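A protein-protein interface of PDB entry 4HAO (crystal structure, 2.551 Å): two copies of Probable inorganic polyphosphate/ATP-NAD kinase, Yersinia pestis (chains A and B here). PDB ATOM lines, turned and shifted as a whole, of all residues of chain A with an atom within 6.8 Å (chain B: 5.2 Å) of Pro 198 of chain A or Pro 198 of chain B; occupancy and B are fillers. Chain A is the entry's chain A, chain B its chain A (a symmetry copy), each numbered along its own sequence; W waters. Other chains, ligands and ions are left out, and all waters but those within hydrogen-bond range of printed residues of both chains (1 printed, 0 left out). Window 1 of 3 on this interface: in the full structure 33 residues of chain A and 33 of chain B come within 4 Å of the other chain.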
ATOM      1  N   SER A 188      -6.776  32.309   7.394  1.00  0.00           N
ATOM      2  CA  SER A 188      -8.224  32.524   7.320  1.00  0.00           C
ATOM      3  C   SER A 188      -8.641  33.919   7.775  1.00  0.00           C
ATOM      4  O   SER A 188      -9.620  34.460   7.291  1.00  0.00           O
ATOM      5  CB  SER A 188      -8.975  31.462   8.121  1.00  0.00           C
ATOM      6  OG  SER A 188      -8.910  31.736   9.516  1.00  0.00           O
ATOM      7  N   THR A 189      -7.872  34.511   8.678  1.00  0.00           N
ATOM      8  CA  THR A 189      -8.140  35.867   9.130  1.00  0.00           C
ATOM      9  C   THR A 189      -7.454  36.904   8.250  1.00  0.00           C
ATOM     10  O   THR A 189      -7.516  38.108   8.524  1.00  0.00           O
ATOM     11  CB  THR A 189      -7.692  36.066  10.582  1.00  0.00           C
ATOM     12  OG1 THR A 189      -6.357  35.569  10.743  1.00  0.00           O
ATOM     13  CG2 THR A 189      -8.603  35.302  11.510  1.00  0.00           C
ATOM     14  N   SER A 192      -7.996  35.895   2.690  1.00  0.00           N
ATOM     15  CA  SER A 192      -9.213  35.080   2.591  1.00  0.00           C
ATOM     16  C   SER A 192     -10.470  35.674   3.260  1.00  0.00           C
ATOM     17  O   SER A 192     -11.576  35.635   2.700  1.00  0.00           O
ATOM     18  CB  SER A 192      -8.944  33.718   3.187  1.00  0.00           C
ATOM     19  OG  SER A 192      -9.984  32.866   2.814  1.00  0.00           O
ATOM     20  N   LEU A 193     -10.293  36.205   4.469  1.00  0.00           N
ATOM     21  CA  LEU A 193     -11.362  36.901   5.161  1.00  0.00           C
ATOM     22  C   LEU A 193     -11.928  38.009   4.289  1.00  0.00           C
ATOM     23  O   LEU A 193     -13.125  38.064   4.061  1.00  0.00           O
ATOM     24  CB  LEU A 193     -10.848  37.484   6.485  1.00  0.00           C
ATOM     25  CG  LEU A 193     -11.904  37.903   7.514  1.00  0.00           C
ATOM     26  CD1 LEU A 193     -12.729  36.696   7.891  1.00  0.00           C
ATOM     27  CD2 LEU A 193     -11.251  38.507   8.744  1.00  0.00           C
ATOM     28  N   GLY A 196     -14.375  37.236   1.721  1.00  0.00           N
ATOM     29  CA  GLY A 196     -15.645  36.657   2.129  1.00  0.00           C
ATOM     30  C   GLY A 196     -15.553  35.239   2.669  1.00  0.00           C
ATOM     31  O   GLY A 196     -16.552  34.542   2.776  1.00  0.00           O
ATOM     32  N   GLY A 197     -14.348  34.800   2.988  1.00  0.00           N
ATOM     33  CA  GLY A 197     -14.147  33.482   3.544  1.00  0.00           C
ATOM     34  C   GLY A 197     -14.446  33.510   5.037  1.00  0.00           C
ATOM     35  O   GLY A 197     -14.521  34.598   5.630  1.00  0.00           O
ATOM     36  N   PRO A 198     -14.635  32.316   5.640  1.00  0.00           N
ATOM     37  CA  PRO A 198     -14.889  32.117   7.063  1.00  0.00           C
ATOM     38  C   PRO A 198     -13.635  32.067   7.887  1.00  0.00           C
ATOM     39  O   PRO A 198     -12.612  31.632   7.392  1.00  0.00           O
ATOM     40  CB  PRO A 198     -15.509  30.720   7.095  1.00  0.00           C
ATOM     41  CG  PRO A 198     -14.845  30.011   5.934  1.00  0.00           C
ATOM     42  CD  PRO A 198     -14.776  31.058   4.877  1.00  0.00           C
ATOM     43  N   ILE A 199     -13.739  32.436   9.156  1.00  0.00           N
ATOM     44  CA  ILE A 199     -12.666  32.223  10.124  1.00  0.00           C
ATOM     45  C   ILE A 199     -12.530  30.761  10.557  1.00  0.00           C
ATOM     46  O   ILE A 199     -13.507  30.160  11.044  1.00  0.00           O
ATOM     47  CB  ILE A 199     -12.962  33.017  11.374  1.00  0.00           C
ATOM     48  CG1 ILE A 199     -13.229  34.465  11.004  1.00  0.00           C
ATOM     49  CG2 ILE A 199     -11.837  32.887  12.367  1.00  0.00           C
ATOM     50  CD1 ILE A 199     -13.776  35.252  12.130  1.00  0.00           C
ATOM     51  N   LEU A 200     -11.333  30.189  10.391  1.00  0.00           N
ATOM     52  CA  LEU A 200     -11.024  28.880  10.988  1.00  0.00           C
ATOM     53  C   LEU A 200     -10.205  29.051  12.256  1.00  0.00           C
ATOM     54  O   LEU A 200      -9.336  29.902  12.339  1.00  0.00           O
ATOM     55  CB  LEU A 200     -10.274  27.921  10.042  1.00  0.00           C
ATOM     56  CG  LEU A 200     -10.588  27.853   8.544  1.00  0.00           C
ATOM     57  CD1 LEU A 200      -9.819  26.729   7.850  1.00  0.00           C
ATOM     58  CD2 LEU A 200     -12.064  27.747   8.281  1.00  0.00           C
ATOM     59  N   VAL A 208      -9.153  26.116   3.662  1.00  0.00           N
ATOM     60  CA  VAL A 208     -10.316  26.689   3.010  1.00  0.00           C
ATOM     61  C   VAL A 208     -10.012  27.218   1.607  1.00  0.00           C
ATOM     62  O   VAL A 208      -9.041  27.928   1.387  1.00  0.00           O
ATOM     63  CB  VAL A 208     -10.956  27.804   3.873  1.00  0.00           C
ATOM     64  CG1 VAL A 208     -10.004  29.008   4.031  1.00  0.00           C
ATOM     65  CG2 VAL A 208     -12.268  28.233   3.271  1.00  0.00           C
ATOM     66  N   LEU A 209     -10.861  26.862   0.654  1.00  0.00           N
ATOM     67  CA  LEU A 209     -10.753  27.361  -0.719  1.00  0.00           C
ATOM     68  C   LEU A 209     -11.793  28.449  -0.937  1.00  0.00           C
ATOM     69  O   LEU A 209     -12.983  28.229  -0.711  1.00  0.00           O
ATOM     70  CB  LEU A 209     -11.000  26.230  -1.722  1.00  0.00           C
ATOM     71  CG  LEU A 209      -9.973  25.106  -1.857  1.00  0.00           C
ATOM     72  CD1 LEU A 209      -9.871  24.281  -0.607  1.00  0.00           C
ATOM     73  CD2 LEU A 209     -10.344  24.224  -3.021  1.00  0.00           C
ATOM     74  N   VAL A 210     -11.357  29.622  -1.375  1.00  0.00           N
ATOM     75  CA  VAL A 210     -12.280  30.730  -1.576  1.00  0.00           C
ATOM     76  C   VAL A 210     -12.099  31.264  -2.971  1.00  0.00           C
ATOM     77  O   VAL A 210     -11.018  31.671  -3.332  1.00  0.00           O
ATOM     78  CB  VAL A 210     -12.041  31.881  -0.558  1.00  0.00           C
ATOM     79  CG1 VAL A 210     -12.859  33.108  -0.922  1.00  0.00           C
ATOM     80  CG2 VAL A 210     -12.396  31.422   0.854  1.00  0.00           C
ATOM     81  N   ARG A 220     -19.106  29.113  -3.179  1.00  0.00           N
ATOM     82  CA  ARG A 220     -19.071  29.287  -1.727  1.00  0.00           C
ATOM     83  C   ARG A 220     -17.723  28.788  -1.220  1.00  0.00           C
ATOM     84  O   ARG A 220     -17.163  27.853  -1.796  1.00  0.00           O
ATOM     85  CB  ARG A 220     -20.184  28.462  -1.042  1.00  0.00           C
ATOM     86  CG  ARG A 220     -21.606  29.005  -1.157  1.00  0.00           C
ATOM     87  CD  ARG A 220     -21.718  30.430  -0.623  1.00  0.00           C
ATOM     88  NE  ARG A 220     -23.088  30.929  -0.726  1.00  0.00           N
ATOM     89  CZ  ARG A 220     -23.696  31.248  -1.874  1.00  0.00           C
ATOM     90  NH1 ARG A 220     -23.057  31.125  -3.035  1.00  0.00           N
ATOM     91  NH2 ARG A 220     -24.950  31.700  -1.868  1.00  0.00           N
ATOM     92  N   PRO A 221     -17.205  29.392  -0.134  1.00  0.00           N
ATOM     93  CA  PRO A 221     -15.989  28.867   0.491  1.00  0.00           C
ATOM     94  C   PRO A 221     -16.139  27.388   0.814  1.00  0.00           C
ATOM     95  O   PRO A 221     -17.173  26.970   1.340  1.00  0.00           O
ATOM     96  CB  PRO A 221     -15.871  29.690   1.770  1.00  0.00           C
ATOM     97  CG  PRO A 221     -16.534  30.981   1.431  1.00  0.00           C
ATOM     98  CD  PRO A 221     -17.650  30.647   0.496  1.00  0.00           C
ATOM     99  N   LEU A 222     -15.121  26.604   0.457  1.00  0.00           N
ATOM    100  CA  LEU A 222     -15.125  25.165   0.693  1.00  0.00           C
ATOM    101  C   LEU A 222     -14.078  24.860   1.741  1.00  0.00           C
ATOM    102  O   LEU A 222     -12.915  25.187   1.551  1.00  0.00           O
ATOM    103  CB  LEU A 222     -14.794  24.422  -0.600  1.00  0.00           C
ATOM    104  CG  LEU A 222     -14.613  22.904  -0.517  1.00  0.00           C
ATOM    105  CD1 LEU A 222     -15.944  22.206  -0.213  1.00  0.00           C
ATOM    106  CD2 LEU A 222     -14.052  22.375  -1.806  1.00  0.00           C
ATOM    107  N   VAL A 223     -14.474  24.268   2.859  1.00  0.00           N
ATOM    108  CA  VAL A 223     -13.488  23.890   3.869  1.00  0.00           C
ATOM    109  C   VAL A 223     -13.219  22.397   3.787  1.00  0.00           C
ATOM    110  O   VAL A 223     -14.152  21.575   3.971  1.00  0.00           O
ATOM    111  CB  VAL A 223     -13.935  24.236   5.319  1.00  0.00           C
ATOM    112  CG1 VAL A 223     -12.807  23.979   6.298  1.00  0.00           C
ATOM    113  CG2 VAL A 223     -14.366  25.678   5.414  1.00  0.00           C
ATOM    114  N   SER B 188     -23.811  21.557   6.895  1.00  0.00           N
ATOM    115  CA  SER B 188     -23.218  22.730   6.247  1.00  0.00           C
ATOM    116  C   SER B 188     -23.858  23.050   4.900  1.00  0.00           C
ATOM    117  O   SER B 188     -23.920  24.200   4.503  1.00  0.00           O
ATOM    118  CB  SER B 188     -21.709  22.560   6.087  1.00  0.00           C
ATOM    119  OG  SER B 188     -21.406  21.690   5.002  1.00  0.00           O
ATOM    120  N   LEU B 193     -25.956  26.853   5.037  1.00  0.00           N
ATOM    121  CA  LEU B 193     -25.629  27.363   3.718  1.00  0.00           C
ATOM    122  C   LEU B 193     -26.489  28.569   3.385  1.00  0.00           C
ATOM    123  O   LEU B 193     -25.972  29.619   3.039  1.00  0.00           O
ATOM    124  CB  LEU B 193     -25.828  26.267   2.660  1.00  0.00           C
ATOM    125  CG  LEU B 193     -25.170  26.495   1.295  1.00  0.00           C
ATOM    126  CD1 LEU B 193     -23.677  26.618   1.482  1.00  0.00           C
ATOM    127  CD2 LEU B 193     -25.495  25.360   0.341  1.00  0.00           C
ATOM    128  N   GLY B 196     -25.588  31.852   4.647  1.00  0.00           N
ATOM    129  CA  GLY B 196     -24.311  32.420   4.245  1.00  0.00           C
ATOM    130  C   GLY B 196     -23.092  31.710   4.812  1.00  0.00           C
ATOM    131  O   GLY B 196     -21.991  32.241   4.792  1.00  0.00           O
ATOM    132  N   GLY B 197     -23.292  30.516   5.343  1.00  0.00           N
ATOM    133  CA  GLY B 197     -22.201  29.737   5.879  1.00  0.00           C
ATOM    134  C   GLY B 197     -21.480  29.024   4.742  1.00  0.00           C
ATOM    135  O   GLY B 197     -22.022  28.937   3.628  1.00  0.00           O
ATOM    136  N   PRO B 198     -20.252  28.531   5.016  1.00  0.00           N
ATOM    137  CA  PRO B 198     -19.413  27.781   4.087  1.00  0.00           C
ATOM    138  C   PRO B 198     -19.733  26.315   4.052  1.00  0.00           C
ATOM    139  O   PRO B 198     -20.154  25.772   5.056  1.00  0.00           O
ATOM    140  CB  PRO B 198     -18.024  27.928   4.706  1.00  0.00           C
ATOM    141  CG  PRO B 198     -18.304  28.014   6.191  1.00  0.00           C
ATOM    142  CD  PRO B 198     -19.534  28.851   6.268  1.00  0.00           C
ATOM    143  N   ILE B 199     -19.460  25.670   2.927  1.00  0.00           N
ATOM    144  CA  ILE B 199     -19.504  24.214   2.827  1.00  0.00           C
ATOM    145  C   ILE B 199     -18.318  23.529   3.511  1.00  0.00           C
ATOM    146  O   ILE B 199     -17.153  23.824   3.184  1.00  0.00           O
ATOM    147  CB  ILE B 199     -19.452  23.815   1.372  1.00  0.00           C
ATOM    148  CG1 ILE B 199     -20.532  24.555   0.603  1.00  0.00           C
ATOM    149  CG2 ILE B 199     -19.577  22.321   1.224  1.00  0.00           C
ATOM    150  CD1 ILE B 199     -20.387  24.420  -0.862  1.00  0.00           C
ATOM    151  N   LEU B 200     -18.602  22.619   4.449  1.00  0.00           N
ATOM    152  CA  LEU B 200     -17.560  21.734   4.993  1.00  0.00           C
ATOM    153  C   LEU B 200     -17.638  20.360   4.352  1.00  0.00           C
ATOM    154  O   LEU B 200     -18.710  19.839   4.097  1.00  0.00           O
ATOM    155  CB  LEU B 200     -17.617  21.568   6.526  1.00  0.00           C
ATOM    156  CG  LEU B 200     -17.979  22.733   7.452  1.00  0.00           C
ATOM    157  CD1 LEU B 200     -17.825  22.358   8.926  1.00  0.00           C
ATOM    158  CD2 LEU B 200     -17.204  23.978   7.122  1.00  0.00           C
ATOM    159  N   VAL B 208     -19.354  24.372  12.385  1.00  0.00           N
ATOM    160  CA  VAL B 208     -19.406  25.773  12.010  1.00  0.00           C
ATOM    161  C   VAL B 208     -20.510  26.543  12.737  1.00  0.00           C
ATOM    162  O   VAL B 208     -21.650  26.107  12.814  1.00  0.00           O
ATOM    163  CB  VAL B 208     -19.558  25.943  10.479  1.00  0.00           C
ATOM    164  CG1 VAL B 208     -20.910  25.388   9.983  1.00  0.00           C
ATOM    165  CG2 VAL B 208     -19.403  27.393  10.103  1.00  0.00           C
ATOM    166  N   VAL B 210     -22.737  29.937  12.702  1.00  0.00           N
ATOM    167  CA  VAL B 210     -23.143  30.988  11.779  1.00  0.00           C
ATOM    168  C   VAL B 210     -24.182  31.846  12.450  1.00  0.00           C
ATOM    169  O   VAL B 210     -25.210  31.353  12.856  1.00  0.00           O
ATOM    170  CB  VAL B 210     -23.736  30.412  10.463  1.00  0.00           C
ATOM    171  CG1 VAL B 210     -24.352  31.512   9.615  1.00  0.00           C
ATOM    172  CG2 VAL B 210     -22.653  29.689   9.665  1.00  0.00           C
ATOM    173  N   PRO B 221     -18.924  33.472   9.741  1.00  0.00           N
ATOM    174  CA  PRO B 221     -18.946  32.059  10.125  1.00  0.00           C
ATOM    175  C   PRO B 221     -17.636  31.653  10.782  1.00  0.00           C
ATOM    176  O   PRO B 221     -16.560  32.005  10.291  1.00  0.00           O
ATOM    177  CB  PRO B 221     -19.128  31.339   8.793  1.00  0.00           C
ATOM    178  CG  PRO B 221     -19.865  32.321   7.949  1.00  0.00           C
ATOM    179  CD  PRO B 221     -19.376  33.673   8.354  1.00  0.00           C
ATOM    180  N   VAL B 223     -15.412  28.459  12.023  1.00  0.00           N
ATOM    181  CA  VAL B 223     -15.270  27.006  11.966  1.00  0.00           C
ATOM    182  C   VAL B 223     -14.333  26.540  13.067  1.00  0.00           C
ATOM    183  O   VAL B 223     -13.143  26.947  13.099  1.00  0.00           O
ATOM    184  CB  VAL B 223     -14.723  26.498  10.600  1.00  0.00           C
ATOM    185  CG1 VAL B 223     -14.761  24.984  10.542  1.00  0.00           C
ATOM    186  CG2 VAL B 223     -15.530  27.066   9.460  1.00  0.00           C
HETATM  187  O   HOH W   1     -23.593  30.045   1.867  1.00  0.00           O
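The backbone NH (N) of Ile 199 of chain A lies within hydrogen-bond range of the backbone carbonyl oxygen (O) of Pro 221 of chain B, at 3.1 Å. O of Ile 199 of chain A is in hydrogen-bond range of N of Val 223 of chain B (2.7 Å). The backbone carbonyl oxygen (O) of Pro 221 of chain A is in hydrogen-bond range of the backbone NH (N) of Ile 199 of chain B, at 3.1 Å. O of Ile 199 of chain B lies within hydrogen-bond range of N of Val 223 of chain A (2.7 Å).
The side-chain hydroxyl (OG) of Ser 188 of chain A lies within hydrogen-bond range of the backbone NH (N) of Leu 200 of chain A. The backbone NH of Leu 209 of chain A is in hydrogen-bond range of the backbone carbonyl oxygen of Leu 222 of chain A (2.8 Å). The side-chain hydroxyl (OG) of Ser 188 of chain B is in hydrogen-bond range of the backbone NH (N) of Leu 200 of chain B (3.0 Å).
Among the printed residues, pairs that only touch across the chains: Pro 198 of chain A with Pro 198 of chain B (3.99 Å), Pro 198 of chain A with Pro 221 of chain B (3.6 Å), Leu 200 of chain A with Val 223 of chain B (3.6 Å), Pro 221 of chain A with Pro 198 of chain B (3.6 Å), Leu 222 of chain A with Ile 199 of chain B (3.5 Å) and Val 223 of chain A with Leu 200 of chain B (3.6 Å).
Printed residues of chain B within 4 Å of Pro 198 of chain A: Pro 198 and Pro 221. Printed residues of chain B within 4 Å of Leu 200 of chain A: Val 223. Of the printed residues of chain B, Pro 221 of chain A touches Pro 198 and Ile 199. Of the printed residues of chain B, Leu 222 of chain A touches Ile 199. Ser 188 of chain B touches none of the printed residues of chain A. Printed residues of chain A within 4 Å of Pro 198 of chain B: Pro 198 and Pro 221. Of the printed residues of chain A, Ile 199 of chain B touches Pro 221 (3.1 Å), Leu 222 (3.5 Å) and Val 223 (2.7 Å). Of the printed residues of chain A, Pro 221 of chain B touches Pro 198 (3.6 Å) and Ile 199 (3.1 Å). The nearest printed residue of chain B that does not touch Pro 198 of chain A is Val 223 of chain B (4.4 Å). The nearest printed residue of chain B that does not touch Ile 199 of chain A is Val 208 of chain B (6.6 Å).
Hydrophobic or aromatic side chains of chain A that line the printed part of chain B: Pro 198, Ile 199, Leu 200, Leu 222 and Val 223. Of the 11 printed residues of chain B, 5 touch a printed residue of chain A. Printed residues of chain B that touch a printed residue of chain A: Pro 198, Ile 199, Leu 200, Pro 221 and Val 223. Hydrophobic or aromatic side chains of chain B within 4 Å of the printed part of chain A: Pro 198, Ile 199, Leu 200 and Val 223.
Pro 198 of chain B touches its own counterpart, Pro 198 of chain A. Pro 198 of chain A touches Pro 221 of chain B, and with the chains exchanged Pro 221 of chain A touches Pro 198 of chain B. Ile 199 of chain A touches Val 223 of chain B, and with the chains exchanged Val 223 of chain A touches Ile 199 of chain B. Leu 200 of chain A touches Val 223 of chain B, and with the chains exchanged Val 223 of chain A touches Leu 200 of chain B. Positions printed for both chains: 188, 193, 196, 197, 198, 199, 200, 208, 210, 221 and 223.
Water W1 lies within hydrogen-bond range of O of Gly 197 of chain B, O of Leu 193 of chain B and NE of Arg 220 of chain A.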
